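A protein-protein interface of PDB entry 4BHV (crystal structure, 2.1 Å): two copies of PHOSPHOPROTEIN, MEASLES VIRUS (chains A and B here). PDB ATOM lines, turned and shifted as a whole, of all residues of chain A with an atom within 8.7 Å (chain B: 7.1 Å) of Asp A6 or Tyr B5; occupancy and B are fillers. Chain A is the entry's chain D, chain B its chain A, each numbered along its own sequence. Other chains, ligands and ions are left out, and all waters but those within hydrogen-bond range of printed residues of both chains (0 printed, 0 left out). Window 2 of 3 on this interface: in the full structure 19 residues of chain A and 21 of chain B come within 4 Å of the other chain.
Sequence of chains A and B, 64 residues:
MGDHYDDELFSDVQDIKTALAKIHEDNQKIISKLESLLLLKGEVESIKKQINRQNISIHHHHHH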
ATOM      1  N   TYR A   5      -5.802  -6.255 -16.284  1.00  0.00           N
ATOM      2  CA  TYR A   5      -6.818  -5.313 -16.718  1.00  0.00           C
ATOM      3  C   TYR A   5      -6.665  -4.030 -15.918  1.00  0.00           C
ATOM      4  O   TYR A   5      -7.058  -3.967 -14.760  1.00  0.00           O
ATOM      5  CB  TYR A   5      -8.201  -5.913 -16.474  1.00  0.00           C
ATOM      6  CG  TYR A   5      -9.300  -5.329 -17.318  1.00  0.00           C
ATOM      7  CD1 TYR A   5      -9.205  -4.048 -17.833  1.00  0.00           C
ATOM      8  CD2 TYR A   5     -10.445  -6.064 -17.599  1.00  0.00           C
ATOM      9  CE1 TYR A   5     -10.215  -3.515 -18.608  1.00  0.00           C
ATOM     10  CE2 TYR A   5     -11.462  -5.539 -18.370  1.00  0.00           C
ATOM     11  CZ  TYR A   5     -11.345  -4.263 -18.874  1.00  0.00           C
ATOM     12  OH  TYR A   5     -12.354  -3.744 -19.645  1.00  0.00           O
ATOM     13  N   ASP A   6      -6.067  -3.014 -16.527  1.00  0.00           N
ATOM     14  CA  ASP A   6      -5.851  -1.735 -15.861  1.00  0.00           C
ATOM     15  C   ASP A   6      -7.153  -0.988 -15.570  1.00  0.00           C
ATOM     16  O   ASP A   6      -8.041  -0.911 -16.408  1.00  0.00           O
ATOM     17  CB  ASP A   6      -4.910  -0.862 -16.691  1.00  0.00           C
ATOM     18  CG  ASP A   6      -4.733   0.519 -16.107  1.00  0.00           C
ATOM     19  OD1 ASP A   6      -3.949   0.658 -15.152  1.00  0.00           O
ATOM     20  OD2 ASP A   6      -5.375   1.465 -16.604  1.00  0.00           O
ATOM     21  N   ASP A   7      -7.240  -0.420 -14.373  1.00  0.00           N
ATOM     22  CA  ASP A   7      -8.448   0.247 -13.901  1.00  0.00           C
ATOM     23  C   ASP A   7      -8.843   1.465 -14.738  1.00  0.00           C
ATOM     24  O   ASP A   7     -10.023   1.689 -14.989  1.00  0.00           O
ATOM     25  CB  ASP A   7      -8.339   0.593 -12.411  1.00  0.00           C
ATOM     26  CG  ASP A   7      -8.101  -0.632 -11.540  1.00  0.00           C
ATOM     27  OD1 ASP A   7      -8.755  -1.668 -11.760  1.00  0.00           O
ATOM     28  OD2 ASP A   7      -7.256  -0.555 -10.628  1.00  0.00           O
ATOM     29  N   GLU A   8      -7.853   2.232 -15.182  1.00  0.00           N
ATOM     30  CA  GLU A   8      -8.106   3.336 -16.097  1.00  0.00           C
ATOM     31  C   GLU A   8      -8.684   2.811 -17.409  1.00  0.00           C
ATOM     32  O   GLU A   8      -9.632   3.368 -17.952  1.00  0.00           O
ATOM     33  CB  GLU A   8      -6.817   4.120 -16.371  1.00  0.00           C
ATOM     34  CG  GLU A   8      -6.510   5.207 -15.348  1.00  0.00           C
ATOM     35  CD  GLU A   8      -5.128   5.824 -15.511  1.00  0.00           C
ATOM     36  OE1 GLU A   8      -4.319   5.310 -16.308  1.00  0.00           O
ATOM     37  OE2 GLU A   8      -4.847   6.830 -14.834  1.00  0.00           O
ATOM     38  N   LEU A   9      -8.109   1.725 -17.907  1.00  0.00           N
ATOM     39  CA  LEU A   9      -8.573   1.098 -19.140  1.00  0.00           C
ATOM     40  C   LEU A   9     -10.012   0.587 -18.974  1.00  0.00           C
ATOM     41  O   LEU A   9     -10.822   0.666 -19.886  1.00  0.00           O
ATOM     42  CB  LEU A   9      -7.614  -0.012 -19.566  1.00  0.00           C
ATOM     43  CG  LEU A   9      -7.964  -0.827 -20.810  1.00  0.00           C
ATOM     44  CD1 LEU A   9      -8.158   0.067 -22.018  1.00  0.00           C
ATOM     45  CD2 LEU A   9      -6.919  -1.894 -21.065  1.00  0.00           C
ATOM     46  N   PHE A  10     -10.325   0.083 -17.787  1.00  0.00           N
ATOM     47  CA  PHE A  10     -11.663  -0.409 -17.504  1.00  0.00           C
ATOM     48  C   PHE A  10     -12.706   0.703 -17.609  1.00  0.00           C
ATOM     49  O   PHE A  10     -13.766   0.498 -18.177  1.00  0.00           O
ATOM     50  CB  PHE A  10     -11.706  -1.056 -16.118  1.00  0.00           C
ATOM     51  CG  PHE A  10     -13.060  -1.560 -15.723  1.00  0.00           C
ATOM     52  CD1 PHE A  10     -13.494  -2.811 -16.129  1.00  0.00           C
ATOM     53  CD2 PHE A  10     -13.897  -0.789 -14.939  1.00  0.00           C
ATOM     54  CE1 PHE A  10     -14.736  -3.282 -15.763  1.00  0.00           C
ATOM     55  CE2 PHE A  10     -15.139  -1.253 -14.568  1.00  0.00           C
ATOM     56  CZ  PHE A  10     -15.561  -2.501 -14.981  1.00  0.00           C
ATOM     57  N   SER A  11     -12.382   1.883 -17.087  1.00  0.00           N
ATOM     58  CA  SER A  11     -13.275   3.027 -17.169  1.00  0.00           C
ATOM     59  C   SER A  11     -13.527   3.412 -18.616  1.00  0.00           C
ATOM     60  O   SER A  11     -14.655   3.684 -19.004  1.00  0.00           O
ATOM     61  CB  SER A  11     -12.646   4.224 -16.459  1.00  0.00           C
ATOM     62  OG  SER A  11     -13.098   4.328 -15.131  1.00  0.00           O
ATOM     63  N   ASP A  12     -12.465   3.429 -19.408  1.00  0.00           N
ATOM     64  CA  ASP A  12     -12.562   3.775 -20.815  1.00  0.00           C
ATOM     65  C   ASP A  12     -13.434   2.772 -21.589  1.00  0.00           C
ATOM     66  O   ASP A  12     -14.214   3.156 -22.448  1.00  0.00           O
ATOM     67  CB  ASP A  12     -11.165   3.937 -21.425  1.00  0.00           C
ATOM     68  CG  ASP A  12     -10.450   5.199 -20.932  1.00  0.00           C
ATOM     69  OD1 ASP A  12     -11.112   6.051 -20.309  1.00  0.00           O
ATOM     70  OD2 ASP A  12      -9.233   5.341 -21.176  1.00  0.00           O
ATOM     71  N   VAL A  13     -13.307   1.491 -21.269  1.00  0.00           N
ATOM     72  CA  VAL A  13     -14.184   0.468 -21.836  1.00  0.00           C
ATOM     73  C   VAL A  13     -15.653   0.653 -21.416  1.00  0.00           C
ATOM     74  O   VAL A  13     -16.565   0.477 -22.217  1.00  0.00           O
ATOM     75  CB  VAL A  13     -13.705  -0.952 -21.494  1.00  0.00           C
ATOM     76  CG1 VAL A  13     -14.730  -1.980 -21.945  1.00  0.00           C
ATOM     77  CG2 VAL A  13     -12.356  -1.228 -22.143  1.00  0.00           C
ATOM     78  N   ILE A  16     -17.136   3.418 -23.415  1.00  0.00           N
ATOM     79  CA  ILE A  16     -17.468   2.988 -24.758  1.00  0.00           C
ATOM     80  C   ILE A  16     -18.827   2.298 -24.756  1.00  0.00           C
ATOM     81  O   ILE A  16     -19.656   2.540 -25.618  1.00  0.00           O
ATOM     82  CB  ILE A  16     -16.386   2.059 -25.334  1.00  0.00           C
ATOM     83  CG1 ILE A  16     -15.153   2.875 -25.747  1.00  0.00           C
ATOM     84  CG2 ILE A  16     -16.927   1.283 -26.523  1.00  0.00           C
ATOM     85  CD1 ILE A  16     -13.852   2.121 -25.683  1.00  0.00           C
ATOM     86  N   TYR B   5      -1.232   0.581 -18.936  1.00  0.00           N
ATOM     87  CA  TYR B   5      -2.062   1.133 -19.982  1.00  0.00           C
ATOM     88  C   TYR B   5      -1.094   1.653 -21.037  1.00  0.00           C
ATOM     89  O   TYR B   5      -0.468   2.696 -20.864  1.00  0.00           O
ATOM     90  CB  TYR B   5      -2.927   2.259 -19.415  1.00  0.00           C
ATOM     91  CG  TYR B   5      -4.166   2.584 -20.209  1.00  0.00           C
ATOM     92  CD1 TYR B   5      -4.253   2.280 -21.556  1.00  0.00           C
ATOM     93  CD2 TYR B   5      -5.252   3.211 -19.607  1.00  0.00           C
ATOM     94  CE1 TYR B   5      -5.392   2.586 -22.282  1.00  0.00           C
ATOM     95  CE2 TYR B   5      -6.394   3.521 -20.317  1.00  0.00           C
ATOM     96  CZ  TYR B   5      -6.462   3.209 -21.658  1.00  0.00           C
ATOM     97  OH  TYR B   5      -7.595   3.517 -22.373  1.00  0.00           O
ATOM     98  N   ASP B   6      -0.937   0.895 -22.117  1.00  0.00           N
ATOM     99  CA  ASP B   6       0.009   1.240 -23.169  1.00  0.00           C
ATOM    100  C   ASP B   6      -0.401   2.545 -23.847  1.00  0.00           C
ATOM    101  O   ASP B   6      -1.583   2.794 -24.041  1.00  0.00           O
ATOM    102  CB  ASP B   6       0.103   0.103 -24.188  1.00  0.00           C
ATOM    103  CG  ASP B   6       1.314   0.228 -25.099  1.00  0.00           C
ATOM    104  OD1 ASP B   6       1.260   1.015 -26.062  1.00  0.00           O
ATOM    105  OD2 ASP B   6       2.311  -0.467 -24.859  1.00  0.00           O
ATOM    106  N   ASP B   7       0.584   3.368 -24.202  1.00  0.00           N
ATOM    107  CA  ASP B   7       0.326   4.676 -24.789  1.00  0.00           C
ATOM    108  C   ASP B   7      -0.398   4.585 -26.122  1.00  0.00           C
ATOM    109  O   ASP B   7      -1.273   5.396 -26.413  1.00  0.00           O
ATOM    110  CB  ASP B   7       1.627   5.470 -24.943  1.00  0.00           C
ATOM    111  CG  ASP B   7       1.646   6.332 -26.199  1.00  0.00           C
ATOM    112  OD1 ASP B   7       1.868   5.789 -27.303  1.00  0.00           O
ATOM    113  OD2 ASP B   7       1.445   7.559 -26.081  1.00  0.00           O
ATOM    114  N   GLU B   8      -0.006   3.621 -26.944  1.00  0.00           N
ATOM    115  CA  GLU B   8      -0.688   3.367 -28.207  1.00  0.00           C
ATOM    116  C   GLU B   8      -2.128   2.866 -28.050  1.00  0.00           C
ATOM    117  O   GLU B   8      -2.996   3.196 -28.848  1.00  0.00           O
ATOM    118  CB  GLU B   8       0.128   2.463 -29.118  1.00  0.00           C
ATOM    119  CG  GLU B   8       0.233   2.990 -30.533  1.00  0.00           C
ATOM    120  CD  GLU B   8       0.888   4.356 -30.615  1.00  0.00           C
ATOM    121  OE1 GLU B   8       0.530   5.241 -29.823  1.00  0.00           O
ATOM    122  OE2 GLU B   8       1.758   4.552 -31.486  1.00  0.00           O
ATOM    123  N   LEU B   9      -2.361   2.046 -27.036  1.00  0.00           N
ATOM    124  CA  LEU B   9      -3.696   1.525 -26.763  1.00  0.00           C
ATOM    125  C   LEU B   9      -4.657   2.653 -26.390  1.00  0.00           C
ATOM    126  O   LEU B   9      -5.794   2.697 -26.833  1.00  0.00           O
ATOM    127  CB  LEU B   9      -3.634   0.466 -25.660  1.00  0.00           C
ATOM    128  CG  LEU B   9      -4.957  -0.037 -25.082  1.00  0.00           C
ATOM    129  CD1 LEU B   9      -5.838  -0.653 -26.157  1.00  0.00           C
ATOM    130  CD2 LEU B   9      -4.721  -1.005 -23.936  1.00  0.00           C
ATOM    131  N   PHE B  10      -4.155   3.572 -25.581  1.00  0.00           N
ATOM    132  CA  PHE B  10      -4.899   4.734 -25.145  1.00  0.00           C
ATOM    133  C   PHE B  10      -5.277   5.594 -26.346  1.00  0.00           C
ATOM    134  O   PHE B  10      -6.392   6.071 -26.436  1.00  0.00           O
ATOM    135  CB  PHE B  10      -4.044   5.528 -24.154  1.00  0.00           C
ATOM    136  CG  PHE B  10      -4.664   6.809 -23.695  1.00  0.00           C
ATOM    137  CD1 PHE B  10      -5.677   6.807 -22.746  1.00  0.00           C
ATOM    138  CD2 PHE B  10      -4.236   8.018 -24.209  1.00  0.00           C
ATOM    139  CE1 PHE B  10      -6.245   7.989 -22.315  1.00  0.00           C
ATOM    140  CE2 PHE B  10      -4.800   9.206 -23.784  1.00  0.00           C
ATOM    141  CZ  PHE B  10      -5.809   9.190 -22.835  1.00  0.00           C
ATOM    142  N   SER B  11      -4.351   5.779 -27.275  1.00  0.00           N
ATOM    143  CA  SER B  11      -4.637   6.569 -28.464  1.00  0.00           C
ATOM    144  C   SER B  11      -5.730   5.943 -29.324  1.00  0.00           C
ATOM    145  O   SER B  11      -6.601   6.635 -29.824  1.00  0.00           O
ATOM    146  CB  SER B  11      -3.368   6.777 -29.293  1.00  0.00           C
ATOM    147  OG  SER B  11      -2.426   7.548 -28.578  1.00  0.00           O
ATOM    148  N   VAL B  13      -8.055   3.904 -28.220  1.00  0.00           N
ATOM    149  CA  VAL B  13      -9.273   4.060 -27.436  1.00  0.00           C
ATOM    150  C   VAL B  13      -9.845   5.469 -27.637  1.00  0.00           C
ATOM    151  O   VAL B  13     -11.050   5.646 -27.757  1.00  0.00           O
ATOM    152  CB  VAL B  13      -9.024   3.779 -25.943  1.00  0.00           C
ATOM    153  CG1 VAL B  13     -10.125   4.381 -25.092  1.00  0.00           C
ATOM    154  CG2 VAL B  13      -8.907   2.284 -25.693  1.00  0.00           C
ATOM    155  N   GLN B  14      -8.962   6.458 -27.691  1.00  0.00           N
ATOM    156  CA  GLN B  14      -9.352   7.834 -27.962  1.00  0.00           C
ATOM    157  C   GLN B  14      -9.968   7.962 -29.353  1.00  0.00           C
ATOM    158  O   GLN B  14     -10.946   8.674 -29.538  1.00  0.00           O
ATOM    159  CB  GLN B  14      -8.154   8.766 -27.831  1.00  0.00           C
ATOM    160  CG  GLN B  14      -7.759   9.091 -26.400  1.00  0.00           C
ATOM    161  CD  GLN B  14      -8.957   9.343 -25.504  1.00  0.00           C
ATOM    162  OE1 GLN B  14      -9.690  10.311 -25.690  1.00  0.00           O
ATOM    163  NE2 GLN B  14      -9.157   8.471 -24.528  1.00  0.00           N
ATOM    164  N   LYS B  17     -13.515   6.703 -29.243  1.00  0.00           N
ATOM    165  CA  LYS B  17     -14.411   7.657 -28.607  1.00  0.00           C
ATOM    166  C   LYS B  17     -14.817   8.796 -29.551  1.00  0.00           C
ATOM    167  O   LYS B  17     -15.971   9.182 -29.596  1.00  0.00           O
ATOM    168  CB  LYS B  17     -13.791   8.188 -27.317  1.00  0.00           C
ATOM    169  CG  LYS B  17     -13.746   7.170 -26.191  1.00  0.00           C
ATOM    170  CD  LYS B  17     -13.293   7.796 -24.881  1.00  0.00           C
ATOM    171  CE  LYS B  17     -13.192   6.764 -23.775  1.00  0.00           C
ATOM    172  NZ  LYS B  17     -12.966   7.384 -22.442  1.00  0.00           N
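The side-chain hydroxyl of Tyr B5 is in hydrogen-bond range of the side-chain carboxylate of Asp A12 (2.7 Å).
The side-chain amino group of Lys B17 is in salt-bridge range of the side-chain carboxylate of Asp A12, 3.1 Å away.
The backbone NH (N) of Leu A9 sits at hydrogen-bond distance from the side-chain carboxylate (OD2) of Asp A6, at 3.0 Å.
The side-chain carboxylate of Asp A6 is in hydrogen-bond range of the backbone NH of Glu A8, at 3.0 Å.
OD2 of Asp A6 touches CD2 of Tyr B5, 3.5 Å away.
Tyr B5 touches Glu A8 (CD2 to CB, 3.7 Å).
Leu A9 touches Tyr B5.
CD2 of Leu B9 touches CD2 of Leu A9 (3.7 Å).
CG1 of Val B13 touches CB of Asp A12 (3.8 Å).
Of chain B, only Tyr B5 (3.5 Å) comes within 4 Å of Asp A6.
Of chain A, only Asp A6, Glu A8, Leu A9 and Asp A12 come within 4 Å of Tyr B5.
Of the printed residues of chain B, Asp A12 touches Tyr B5 (2.7 Å), Val B13 (3.8 Å) and Lys B17 (3.1 Å).
Of the printed residues of chain A, Val B13 touches Asp A12.
Phe B10 touches none of the printed residues of chain A.
Asp A7 touches none of the printed residues of chain B.
The nearest residue of chain B that does not touch Asp A6 is Asp B6 (7.0 Å).
Of the 10 printed residues of chain B, 4 touch a printed residue of chain A.
Hydrophobic or aromatic side chains of chain B within 4 Å of the printed part of chain A: Tyr B5, Leu B9 and Val B13.
Along chain B the printed residues that touch a printed residue of chain A span positions 5 to 17.
Hydrophobic or aromatic side chains of chain A within 4 Å of the printed part of chain B: Leu A9.
Among the printed residues, 7 pairs touch across the chains.
Asp A6 touches Tyr B5, but with the chains exchanged Tyr A5 does not touch Asp B6 (9.8 Å).
Glu A8 touches Tyr B5, but with the chains exchanged Tyr A5 does not touch Glu B8 (14.0 Å).
Leu A9 touches Tyr B5, but with the chains exchanged Tyr A5 does not touch Leu B9 (8.1 Å).
Leu B9 touches its own counterpart, Leu A9.
Of the 7 pairs that touch across the chains among the printed residues, 1 has its exchanged pair printed and touching as well.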
